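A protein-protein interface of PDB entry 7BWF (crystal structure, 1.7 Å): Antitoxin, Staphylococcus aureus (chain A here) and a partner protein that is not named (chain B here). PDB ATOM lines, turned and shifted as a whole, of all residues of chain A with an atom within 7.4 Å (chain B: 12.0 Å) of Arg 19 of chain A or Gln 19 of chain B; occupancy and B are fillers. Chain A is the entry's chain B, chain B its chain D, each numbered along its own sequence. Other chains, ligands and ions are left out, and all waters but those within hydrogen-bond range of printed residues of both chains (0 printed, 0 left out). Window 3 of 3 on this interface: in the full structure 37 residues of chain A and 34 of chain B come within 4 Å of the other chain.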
ATOM      1  N   ASN A  14      -2.065  -4.189  -4.046  1.00  0.00           N
ATOM      2  CA  ASN A  14      -1.295  -3.414  -5.005  1.00  0.00           C
ATOM      3  C   ASN A  14      -1.081  -1.997  -4.492  1.00  0.00           C
ATOM      4  O   ASN A  14      -1.703  -1.554  -3.524  1.00  0.00           O
ATOM      5  CB  ASN A  14      -1.965  -3.374  -6.385  1.00  0.00           C
ATOM      6  CG  ASN A  14      -3.355  -2.760  -6.361  1.00  0.00           C
ATOM      7  OD1 ASN A  14      -3.659  -1.872  -5.557  1.00  0.00           O
ATOM      8  ND2 ASN A  14      -4.194  -3.203  -7.283  1.00  0.00           N
ATOM      9  N   TYR A  15      -0.184  -1.283  -5.172  1.00  0.00           N
ATOM     10  CA  TYR A  15       0.317  -0.017  -4.650  1.00  0.00           C
ATOM     11  C   TYR A  15      -0.808   0.987  -4.460  1.00  0.00           C
ATOM     12  O   TYR A  15      -0.881   1.670  -3.436  1.00  0.00           O
ATOM     13  CB  TYR A  15       1.366   0.569  -5.591  1.00  0.00           C
ATOM     14  CG  TYR A  15       1.552   2.067  -5.421  1.00  0.00           C
ATOM     15  CD1 TYR A  15       2.220   2.595  -4.322  1.00  0.00           C
ATOM     16  CD2 TYR A  15       1.059   2.953  -6.368  1.00  0.00           C
ATOM     17  CE1 TYR A  15       2.400   3.967  -4.183  1.00  0.00           C
ATOM     18  CE2 TYR A  15       1.229   4.321  -6.234  1.00  0.00           C
ATOM     19  CZ  TYR A  15       1.898   4.824  -5.137  1.00  0.00           C
ATOM     20  OH  TYR A  15       2.082   6.182  -4.983  1.00  0.00           O
ATOM     21  N   SER A  16      -1.685   1.105  -5.457  1.00  0.00           N
ATOM     22  CA  SER A  16      -2.777   2.070  -5.374  1.00  0.00           C
ATOM     23  C   SER A  16      -3.645   1.786  -4.154  1.00  0.00           C
ATOM     24  O   SER A  16      -3.900   2.672  -3.333  1.00  0.00           O
ATOM     25  CB  SER A  16      -3.614   2.037  -6.658  1.00  0.00           C
ATOM     26  OG  SER A  16      -4.776   1.237  -6.482  1.00  0.00           O
ATOM     27  N   TYR A  17      -4.092   0.537  -4.005  1.00  0.00           N
ATOM     28  CA  TYR A  17      -4.856   0.166  -2.819  1.00  0.00           C
ATOM     29  C   TYR A  17      -4.092   0.522  -1.550  1.00  0.00           C
ATOM     30  O   TYR A  17      -4.639   1.136  -0.627  1.00  0.00           O
ATOM     31  CB  TYR A  17      -5.168  -1.327  -2.848  1.00  0.00           C
ATOM     32  CG  TYR A  17      -5.995  -1.828  -1.686  1.00  0.00           C
ATOM     33  CD1 TYR A  17      -5.399  -2.256  -0.508  1.00  0.00           C
ATOM     34  CD2 TYR A  17      -7.374  -1.900  -1.785  1.00  0.00           C
ATOM     35  CE1 TYR A  17      -6.161  -2.740   0.543  1.00  0.00           C
ATOM     36  CE2 TYR A  17      -8.143  -2.380  -0.745  1.00  0.00           C
ATOM     37  CZ  TYR A  17      -7.533  -2.801   0.421  1.00  0.00           C
ATOM     38  OH  TYR A  17      -8.286  -3.281   1.472  1.00  0.00           O
ATOM     39  N   ALA A  18      -2.811   0.154  -1.495  1.00  0.00           N
ATOM     40  CA  ALA A  18      -2.053   0.317  -0.259  1.00  0.00           C
ATOM     41  C   ALA A  18      -1.899   1.788   0.099  1.00  0.00           C
ATOM     42  O   ALA A  18      -1.970   2.160   1.274  1.00  0.00           O
ATOM     43  CB  ALA A  18      -0.679  -0.350  -0.384  1.00  0.00           C
ATOM     44  N   ARG A  19      -1.681   2.641  -0.899  1.00  0.00           N
ATOM     45  CA  ARG A  19      -1.504   4.060  -0.620  1.00  0.00           C
ATOM     46  C   ARG A  19      -2.804   4.702  -0.158  1.00  0.00           C
ATOM     47  O   ARG A  19      -2.787   5.597   0.691  1.00  0.00           O
ATOM     48  CB  ARG A  19      -0.971   4.781  -1.859  1.00  0.00           C
ATOM     49  CG  ARG A  19      -0.306   6.115  -1.549  1.00  0.00           C
ATOM     50  CD  ARG A  19      -0.327   7.021  -2.769  1.00  0.00           C
ATOM     51  NE  ARG A  19       0.290   8.324  -2.538  1.00  0.00           N
ATOM     52  CZ  ARG A  19      -0.013   9.425  -3.223  1.00  0.00           C
ATOM     53  NH1 ARG A  19      -0.927   9.386  -4.186  1.00  0.00           N
ATOM     54  NH2 ARG A  19       0.601  10.570  -2.949  1.00  0.00           N
ATOM     55  N   GLN A  20      -3.939   4.258  -0.696  1.00  0.00           N
ATOM     56  CA  GLN A  20      -5.225   4.769  -0.235  1.00  0.00           C
ATOM     57  C   GLN A  20      -5.523   4.296   1.184  1.00  0.00           C
ATOM     58  O   GLN A  20      -6.089   5.042   1.990  1.00  0.00           O
ATOM     59  CB  GLN A  20      -6.333   4.317  -1.192  1.00  0.00           C
ATOM     60  CG  GLN A  20      -7.543   5.228  -1.256  1.00  0.00           C
ATOM     61  CD  GLN A  20      -7.225   6.604  -1.796  1.00  0.00           C
ATOM     62  OE1 GLN A  20      -7.256   7.584  -1.057  1.00  0.00           O
ATOM     63  NE2 GLN A  20      -6.937   6.689  -3.093  1.00  0.00           N
ATOM     64  N   ASN A  21      -5.156   3.057   1.510  1.00  0.00           N
ATOM     65  CA  ASN A  21      -5.594   2.434   2.755  1.00  0.00           C
ATOM     66  C   ASN A  21      -4.433   2.165   3.713  1.00  0.00           C
ATOM     67  O   ASN A  21      -4.473   1.209   4.495  1.00  0.00           O
ATOM     68  CB  ASN A  21      -6.335   1.122   2.482  1.00  0.00           C
ATOM     69  CG  ASN A  21      -7.512   1.276   1.528  1.00  0.00           C
ATOM     70  OD1 ASN A  21      -8.451   2.031   1.780  1.00  0.00           O
ATOM     71  ND2 ASN A  21      -7.451   0.557   0.409  1.00  0.00           N
ATOM     72  N   LEU A  22      -3.391   2.994   3.664  1.00  0.00           N
ATOM     73  CA  LEU A  22      -2.186   2.710   4.436  1.00  0.00           C
ATOM     74  C   LEU A  22      -2.510   2.575   5.919  1.00  0.00           C
ATOM     75  O   LEU A  22      -2.097   1.614   6.575  1.00  0.00           O
ATOM     76  CB  LEU A  22      -1.141   3.804   4.207  1.00  0.00           C
ATOM     77  CG  LEU A  22       0.199   3.571   4.913  1.00  0.00           C
ATOM     78  CD1 LEU A  22       0.742   2.182   4.596  1.00  0.00           C
ATOM     79  CD2 LEU A  22       1.177   4.665   4.512  1.00  0.00           C
ATOM     80  N   LYS A  23      -3.254   3.536   6.469  1.00  0.00           N
ATOM     81  CA  LYS A  23      -3.568   3.503   7.895  1.00  0.00           C
ATOM     82  C   LYS A  23      -4.295   2.212   8.262  1.00  0.00           C
ATOM     83  O   LYS A  23      -3.977   1.572   9.271  1.00  0.00           O
ATOM     84  CB  LYS A  23      -4.399   4.731   8.284  1.00  0.00           C
ATOM     85  CG  LYS A  23      -4.312   5.078   9.769  1.00  0.00           C
ATOM     86  CD  LYS A  23      -5.493   5.944  10.211  1.00  0.00           C
ATOM     87  CE  LYS A  23      -5.359   6.347  11.680  1.00  0.00           C
ATOM     88  NZ  LYS A  23      -6.042   5.415  12.627  1.00  0.00           N
ATOM     89  N   LEU A  25      -4.064  -0.629   6.814  1.00  0.00           N
ATOM     90  CA  LEU A  25      -3.113  -1.735   6.739  1.00  0.00           C
ATOM     91  C   LEU A  25      -2.168  -1.723   7.934  1.00  0.00           C
ATOM     92  O   LEU A  25      -1.808  -2.784   8.455  1.00  0.00           O
ATOM     93  CB  LEU A  25      -2.328  -1.664   5.425  1.00  0.00           C
ATOM     94  CG  LEU A  25      -3.171  -1.908   4.173  1.00  0.00           C
ATOM     95  CD1 LEU A  25      -2.341  -1.683   2.910  1.00  0.00           C
ATOM     96  CD2 LEU A  25      -3.777  -3.307   4.176  1.00  0.00           C
ATOM     97  N   VAL A  38       2.916  -5.506  -0.719  1.00  0.00           N
ATOM     98  CA  VAL A  38       2.411  -4.473  -1.609  1.00  0.00           C
ATOM     99  C   VAL A  38       3.134  -4.605  -2.940  1.00  0.00           C
ATOM    100  O   VAL A  38       4.367  -4.513  -2.995  1.00  0.00           O
ATOM    101  CB  VAL A  38       2.615  -3.075  -1.013  1.00  0.00           C
ATOM    102  CG1 VAL A  38       2.128  -2.028  -1.997  1.00  0.00           C
ATOM    103  CG2 VAL A  38       1.895  -2.975   0.316  1.00  0.00           C
ATOM    104  N   LYS B  12      10.151   7.399   9.603  1.00  0.00           N
ATOM    105  CA  LYS B  12       9.248   8.372   9.006  1.00  0.00           C
ATOM    106  C   LYS B  12       7.884   8.257   9.673  1.00  0.00           C
ATOM    107  O   LYS B  12       7.498   7.179  10.133  1.00  0.00           O
ATOM    108  CB  LYS B  12       9.078   8.141   7.498  1.00  0.00           C
ATOM    109  CG  LYS B  12      10.335   8.356   6.677  1.00  0.00           C
ATOM    110  CD  LYS B  12      10.734   9.830   6.621  1.00  0.00           C
ATOM    111  CE  LYS B  12      11.801  10.082   5.559  1.00  0.00           C
ATOM    112  NZ  LYS B  12      12.695  11.214   5.944  1.00  0.00           N
ATOM    113  N   ASN B  13       7.147   9.367   9.716  1.00  0.00           N
ATOM    114  CA  ASN B  13       5.802   9.316  10.273  1.00  0.00           C
ATOM    115  C   ASN B  13       4.793   9.022   9.168  1.00  0.00           C
ATOM    116  O   ASN B  13       5.125   8.964   7.981  1.00  0.00           O
ATOM    117  CB  ASN B  13       5.443  10.613  11.005  1.00  0.00           C
ATOM    118  CG  ASN B  13       5.614  11.850  10.152  1.00  0.00           C
ATOM    119  OD1 ASN B  13       5.369  11.842   8.943  1.00  0.00           O
ATOM    120  ND2 ASN B  13       6.004  12.942  10.795  1.00  0.00           N
ATOM    121  N   TYR B  14       3.534   8.836   9.576  1.00  0.00           N
ATOM    122  CA  TYR B  14       2.574   8.170   8.703  1.00  0.00           C
ATOM    123  C   TYR B  14       2.160   9.061   7.540  1.00  0.00           C
ATOM    124  O   TYR B  14       2.104   8.606   6.393  1.00  0.00           O
ATOM    125  CB  TYR B  14       1.327   7.751   9.478  1.00  0.00           C
ATOM    126  CG  TYR B  14       0.067   7.748   8.618  1.00  0.00           C
ATOM    127  CD1 TYR B  14      -0.259   6.666   7.806  1.00  0.00           C
ATOM    128  CD2 TYR B  14      -0.793   8.840   8.619  1.00  0.00           C
ATOM    129  CE1 TYR B  14      -1.422   6.671   7.033  1.00  0.00           C
ATOM    130  CE2 TYR B  14      -1.946   8.853   7.847  1.00  0.00           C
ATOM    131  CZ  TYR B  14      -2.258   7.766   7.056  1.00  0.00           C
ATOM    132  OH  TYR B  14      -3.403   7.762   6.284  1.00  0.00           O
ATOM    133  N   SER B  15       1.786  10.311   7.827  1.00  0.00           N
ATOM    134  CA  SER B  15       1.357  11.224   6.768  1.00  0.00           C
ATOM    135  C   SER B  15       2.395  11.260   5.657  1.00  0.00           C
ATOM    136  O   SER B  15       2.077  11.136   4.468  1.00  0.00           O
ATOM    137  CB  SER B  15       1.160  12.637   7.329  1.00  0.00           C
ATOM    138  OG  SER B  15       2.435  13.229   7.572  1.00  0.00           O
ATOM    139  N   TYR B  16       3.656  11.417   6.055  1.00  0.00           N
ATOM    140  CA  TYR B  16       4.793  11.374   5.145  1.00  0.00           C
ATOM    141  C   TYR B  16       4.827  10.084   4.330  1.00  0.00           C
ATOM    142  O   TYR B  16       4.996  10.113   3.104  1.00  0.00           O
ATOM    143  CB  TYR B  16       6.065  11.522   5.975  1.00  0.00           C
ATOM    144  CG  TYR B  16       7.315  11.682   5.180  1.00  0.00           C
ATOM    145  CD1 TYR B  16       7.932  10.594   4.581  1.00  0.00           C
ATOM    146  CD2 TYR B  16       7.888  12.931   5.032  1.00  0.00           C
ATOM    147  CE1 TYR B  16       9.077  10.752   3.854  1.00  0.00           C
ATOM    148  CE2 TYR B  16       9.037  13.105   4.312  1.00  0.00           C
ATOM    149  CZ  TYR B  16       9.631  12.018   3.730  1.00  0.00           C
ATOM    150  OH  TYR B  16      10.784  12.196   3.011  1.00  0.00           O
ATOM    151  N   ALA B  17       4.699   8.933   4.993  1.00  0.00           N
ATOM    152  CA  ALA B  17       4.856   7.672   4.273  1.00  0.00           C
ATOM    153  C   ALA B  17       3.751   7.481   3.245  1.00  0.00           C
ATOM    154  O   ALA B  17       3.998   6.960   2.152  1.00  0.00           O
ATOM    155  CB  ALA B  17       4.877   6.491   5.246  1.00  0.00           C
ATOM    156  N   ARG B  18       2.524   7.880   3.583  1.00  0.00           N
ATOM    157  CA  ARG B  18       1.410   7.691   2.664  1.00  0.00           C
ATOM    158  C   ARG B  18       1.517   8.635   1.476  1.00  0.00           C
ATOM    159  O   ARG B  18       1.082   8.298   0.370  1.00  0.00           O
ATOM    160  CB  ARG B  18       0.082   7.907   3.388  1.00  0.00           C
ATOM    161  CG  ARG B  18      -1.128   7.552   2.538  1.00  0.00           C
ATOM    162  CD  ARG B  18      -2.118   8.691   2.523  1.00  0.00           C
ATOM    163  NE  ARG B  18      -3.497   8.256   2.341  1.00  0.00           N
ATOM    164  CZ  ARG B  18      -4.551   8.967   2.727  1.00  0.00           C
ATOM    165  NH1 ARG B  18      -4.382  10.135   3.334  1.00  0.00           N
ATOM    166  NH2 ARG B  18      -5.778   8.504   2.521  1.00  0.00           N
ATOM    167  N   GLN B  19       2.084   9.822   1.685  1.00  0.00           N
ATOM    168  CA  GLN B  19       2.332  10.720   0.567  1.00  0.00           C
ATOM    169  C   GLN B  19       3.464  10.198  -0.309  1.00  0.00           C
ATOM    170  O   GLN B  19       3.385  10.264  -1.541  1.00  0.00           O
ATOM    171  CB  GLN B  19       2.671  12.122   1.076  1.00  0.00           C
ATOM    172  CG  GLN B  19       2.524  13.200   0.021  1.00  0.00           C
ATOM    173  CD  GLN B  19       1.092  13.372  -0.443  1.00  0.00           C
ATOM    174  OE1 GLN B  19       0.181  13.543   0.368  1.00  0.00           O
ATOM    175  NE2 GLN B  19       0.884  13.321  -1.754  1.00  0.00           N
ATOM    176  N   ASN B  20       4.529   9.684   0.304  1.00  0.00           N
ATOM    177  CA  ASN B  20       5.729   9.297  -0.429  1.00  0.00           C
ATOM    178  C   ASN B  20       5.872   7.780  -0.534  1.00  0.00           C
ATOM    179  O   ASN B  20       6.989   7.258  -0.605  1.00  0.00           O
ATOM    180  CB  ASN B  20       6.978   9.887   0.227  1.00  0.00           C
ATOM    181  CG  ASN B  20       6.976  11.409   0.263  1.00  0.00           C
ATOM    182  OD1 ASN B  20       6.567  12.069  -0.692  1.00  0.00           O
ATOM    183  ND2 ASN B  20       7.422  11.970   1.386  1.00  0.00           N
ATOM    184  N   LEU B  21       4.751   7.057  -0.542  1.00  0.00           N
ATOM    185  CA  LEU B  21       4.821   5.604  -0.432  1.00  0.00           C
ATOM    186  C   LEU B  21       5.634   5.006  -1.575  1.00  0.00           C
ATOM    187  O   LEU B  21       6.495   4.149  -1.356  1.00  0.00           O
ATOM    188  CB  LEU B  21       3.414   5.006  -0.388  1.00  0.00           C
ATOM    189  CG  LEU B  21       3.413   3.474  -0.331  1.00  0.00           C
ATOM    190  CD1 LEU B  21       4.149   2.971   0.910  1.00  0.00           C
ATOM    191  CD2 LEU B  21       1.986   2.949  -0.397  1.00  0.00           C
ATOM    192  N   LYS B  22       5.388   5.452  -2.806  1.00  0.00           N
ATOM    193  CA  LYS B  22       6.106   4.873  -3.936  1.00  0.00           C
ATOM    194  C   LYS B  22       7.602   5.157  -3.838  1.00  0.00           C
ATOM    195  O   LYS B  22       8.428   4.293  -4.157  1.00  0.00           O
ATOM    196  CB  LYS B  22       5.548   5.405  -5.256  1.00  0.00           C
ATOM    197  CG  LYS B  22       6.144   4.706  -6.469  1.00  0.00           C
ATOM    198  CD  LYS B  22       5.312   3.509  -6.861  1.00  0.00           C
ATOM    199  CE  LYS B  22       6.127   2.232  -6.818  1.00  0.00           C
ATOM    200  NZ  LYS B  22       5.239   1.081  -7.138  1.00  0.00           N
ATOM    201  N   ALA B  23       7.974   6.356  -3.393  1.00  0.00           N
ATOM    202  CA  ALA B  23       9.392   6.677  -3.260  1.00  0.00           C
ATOM    203  C   ALA B  23      10.054   5.784  -2.213  1.00  0.00           C
ATOM    204  O   ALA B  23      11.201   5.357  -2.380  1.00  0.00           O
ATOM    205  CB  ALA B  23       9.574   8.159  -2.905  1.00  0.00           C
ATOM    206  N   LEU B  24       9.336   5.472  -1.131  1.00  0.00           N
ATOM    207  CA  LEU B  24       9.892   4.605  -0.097  1.00  0.00           C
ATOM    208  C   LEU B  24      10.009   3.166  -0.586  1.00  0.00           C
ATOM    209  O   LEU B  24      10.962   2.467  -0.226  1.00  0.00           O
ATOM    210  CB  LEU B  24       9.031   4.669   1.168  1.00  0.00           C
ATOM    211  CG  LEU B  24       9.052   6.028   1.871  1.00  0.00           C
ATOM    212  CD1 LEU B  24       8.153   6.017   3.105  1.00  0.00           C
ATOM    213  CD2 LEU B  24      10.478   6.434   2.239  1.00  0.00           C
ATOM    214  N   MET B  25       9.059   2.704  -1.405  1.00  0.00           N
ATOM    215  CA  MET B  25       9.156   1.358  -1.963  1.00  0.00           C
ATOM    216  C   MET B  25      10.375   1.235  -2.868  1.00  0.00           C
ATOM    217  O   MET B  25      11.049   0.202  -2.874  1.00  0.00           O
ATOM    218  CB  MET B  25       7.883   1.004  -2.736  1.00  0.00           C
ATOM    219  CG  MET B  25       6.727   0.606  -1.846  1.00  0.00           C
ATOM    220  SD  MET B  25       5.141   1.089  -2.546  1.00  0.00           S
ATOM    221  CE  MET B  25       4.733  -0.344  -3.524  1.00  0.00           C
ATOM    222  N   THR B  26      10.672   2.277  -3.641  1.00  0.00           N
ATOM    223  CA  THR B  26      11.897   2.286  -4.431  1.00  0.00           C
ATOM    224  C   THR B  26      13.124   2.283  -3.528  1.00  0.00           C
ATOM    225  O   THR B  26      14.085   1.552  -3.776  1.00  0.00           O
ATOM    226  CB  THR B  26      11.916   3.507  -5.353  1.00  0.00           C
ATOM    227  OG1 THR B  26      10.812   3.432  -6.260  1.00  0.00           O
ATOM    228  CG2 THR B  26      13.214   3.544  -6.144  1.00  0.00           C
ATOM    229  N   VAL B  35      12.292   1.015   6.507  1.00  0.00           N
ATOM    230  CA  VAL B  35      11.609   2.208   6.980  1.00  0.00           C
ATOM    231  C   VAL B  35      10.633   1.790   8.064  1.00  0.00           C
ATOM    232  O   VAL B  35       9.765   0.938   7.836  1.00  0.00           O
ATOM    233  CB  VAL B  35      10.881   2.942   5.841  1.00  0.00           C
ATOM    234  CG1 VAL B  35      10.155   4.161   6.389  1.00  0.00           C
ATOM    235  CG2 VAL B  35      11.868   3.315   4.745  1.00  0.00           C
ATOM    236  N   VAL B  37       7.629   3.238   9.860  1.00  0.00           N
ATOM    237  CA  VAL B  37       6.607   4.267   9.755  1.00  0.00           C
ATOM    238  C   VAL B  37       5.911   4.374  11.103  1.00  0.00           C
ATOM    239  O   VAL B  37       5.315   3.399  11.580  1.00  0.00           O
ATOM    240  CB  VAL B  37       5.599   3.946   8.645  1.00  0.00           C
ATOM    241  CG1 VAL B  37       4.561   5.055   8.573  1.00  0.00           C
ATOM    242  CG2 VAL B  37       6.325   3.781   7.327  1.00  0.00           C
ATOM    243  N   THR B  38       5.980   5.552  11.718  1.00  0.00           N
ATOM    244  CA  THR B  38       5.406   5.765  13.037  1.00  0.00           C
ATOM    245  C   THR B  38       3.959   6.227  12.945  1.00  0.00           C
ATOM    246  O   THR B  38       3.542   6.868  11.977  1.00  0.00           O
ATOM    247  CB  THR B  38       6.228   6.784  13.832  1.00  0.00           C
ATOM    248  OG1 THR B  38       6.242   8.048  13.162  1.00  0.00           O
ATOM    249  CG2 THR B  38       7.644   6.281  14.014  1.00  0.00           C
ATOM    250  N   VAL B  45       4.787   0.281  11.869  1.00  0.00           N
ATOM    251  CA  VAL B  45       5.107  -0.796  10.943  1.00  0.00           C
ATOM    252  C   VAL B  45       6.542  -0.635  10.458  1.00  0.00           C
ATOM    253  O   VAL B  45       7.146   0.440  10.542  1.00  0.00           O
ATOM    254  CB  VAL B  45       4.139  -0.844   9.735  1.00  0.00           C
ATOM    255  CG1 VAL B  45       2.710  -0.975  10.218  1.00  0.00           C
ATOM    256  CG2 VAL B  45       4.316   0.389   8.844  1.00  0.00           C
ATOM    257  N   ILE B  47       8.699  -1.375   6.883  1.00  0.00           N
ATOM    258  CA  ILE B  47       8.610  -1.650   5.453  1.00  0.00           C
ATOM    259  C   ILE B  47       9.980  -2.094   4.969  1.00  0.00           C
ATOM    260  O   ILE B  47      10.981  -1.395   5.177  1.00  0.00           O
ATOM    261  CB  ILE B  47       8.134  -0.423   4.657  1.00  0.00           C
ATOM    262  CG1 ILE B  47       6.812   0.099   5.222  1.00  0.00           C
ATOM    263  CG2 ILE B  47       7.962  -0.781   3.196  1.00  0.00           C
ATOM    264  CD1 ILE B  47       6.282   1.360   4.544  1.00  0.00           C
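Among the printed residues, pairs that only touch across the chains: Val 38 of chain A with Met 25 of chain B (3.5 Å), Gln 20 of chain A with Arg 18 of chain B (3.5 Å), Leu 22 of chain A with Arg 18 of chain B (3.6 Å), Tyr 15 of chain A with Lys 22 of chain B (3.6 Å), Arg 19 of chain A with Leu 21 of chain B (3.7 Å), Lys 23 of chain A with Tyr 14 of chain B (3.7 Å), Tyr 15 of chain A with Met 25 of chain B (3.7 Å) and Tyr 15 of chain A with Leu 21 of chain B (3.9 Å).
Printed residues of chain B that touch a printed residue of chain A: Tyr 14, Arg 18, Gln 19, Leu 21, Lys 22 and Met 25. Hydrophobic or aromatic side chains of chain B that line the printed part of chain A: Tyr 14, Leu 21 and Met 25. Of the 12 printed residues of chain A, 6 touch a printed residue of chain B. Hydrophobic or aromatic side chains of chain A within 4 Å of the printed part of chain B: Tyr 15, Leu 22 and Val 38. Among the printed residues, 10 pairs touch across the chains.
Gln 19 of chain B touches just one residue of chain A: Arg 19 (3.0 Å). Tyr 15 of chain A touches three residues of chain B. No residue of chain B comes within 4 Å of Ser 16 of chain A. No residue of chain B comes within 4 Å of Ala 18 of chain A. Of chain B, only Arg 18 comes within 4 Å of Gln 20 of chain A. No residue of chain B comes within 4 Å of Asn 21 of chain A. Of chain B, only Arg 18 (3.6 Å) comes within 4 Å of Leu 22 of chain A. Printed residues of chain A within 4 Å of Lys 22 of chain B: Tyr 15. Of the printed residues of chain B, Lys 23 of chain A touches Tyr 14 (3.7 Å). Printed residues of chain A within 4 Å of Met 25 of chain B: Tyr 15 (3.7 Å) and Val 38 (3.5 Å). Printed residues of chain B within 4 Å of Val 38 of chain A: Met 25 (3.5 Å). Of the printed residues of chain A, Arg 18 of chain B touches Arg 19 (3.0 Å), Gln 20 (3.5 Å) and Leu 22 (3.6 Å). Lys 12 of chain B touches none of the printed residues of chain A. Ser 15 of chain B touches none of the printed residues of chain A. The nearest residue of chain B that does not touch Arg 19 of chain A is Asn 20 of chain B (5.2 Å).
O of Arg 18 of chain B lies within hydrogen-bond range of NE of Arg 19 of chain A (3.0 Å). NH2 of Arg 19 of chain A lies close to NE2 of Gln 19 of chain B.
O of Lys 22 of chain B is in hydrogen-bond range of OG1 of Thr 26 of chain B (3.3 Å). The backbone carbonyl oxygen (O) of Thr 38 of chain B lies within hydrogen-bond range of the backbone NH (N) of Tyr 14 of chain B.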
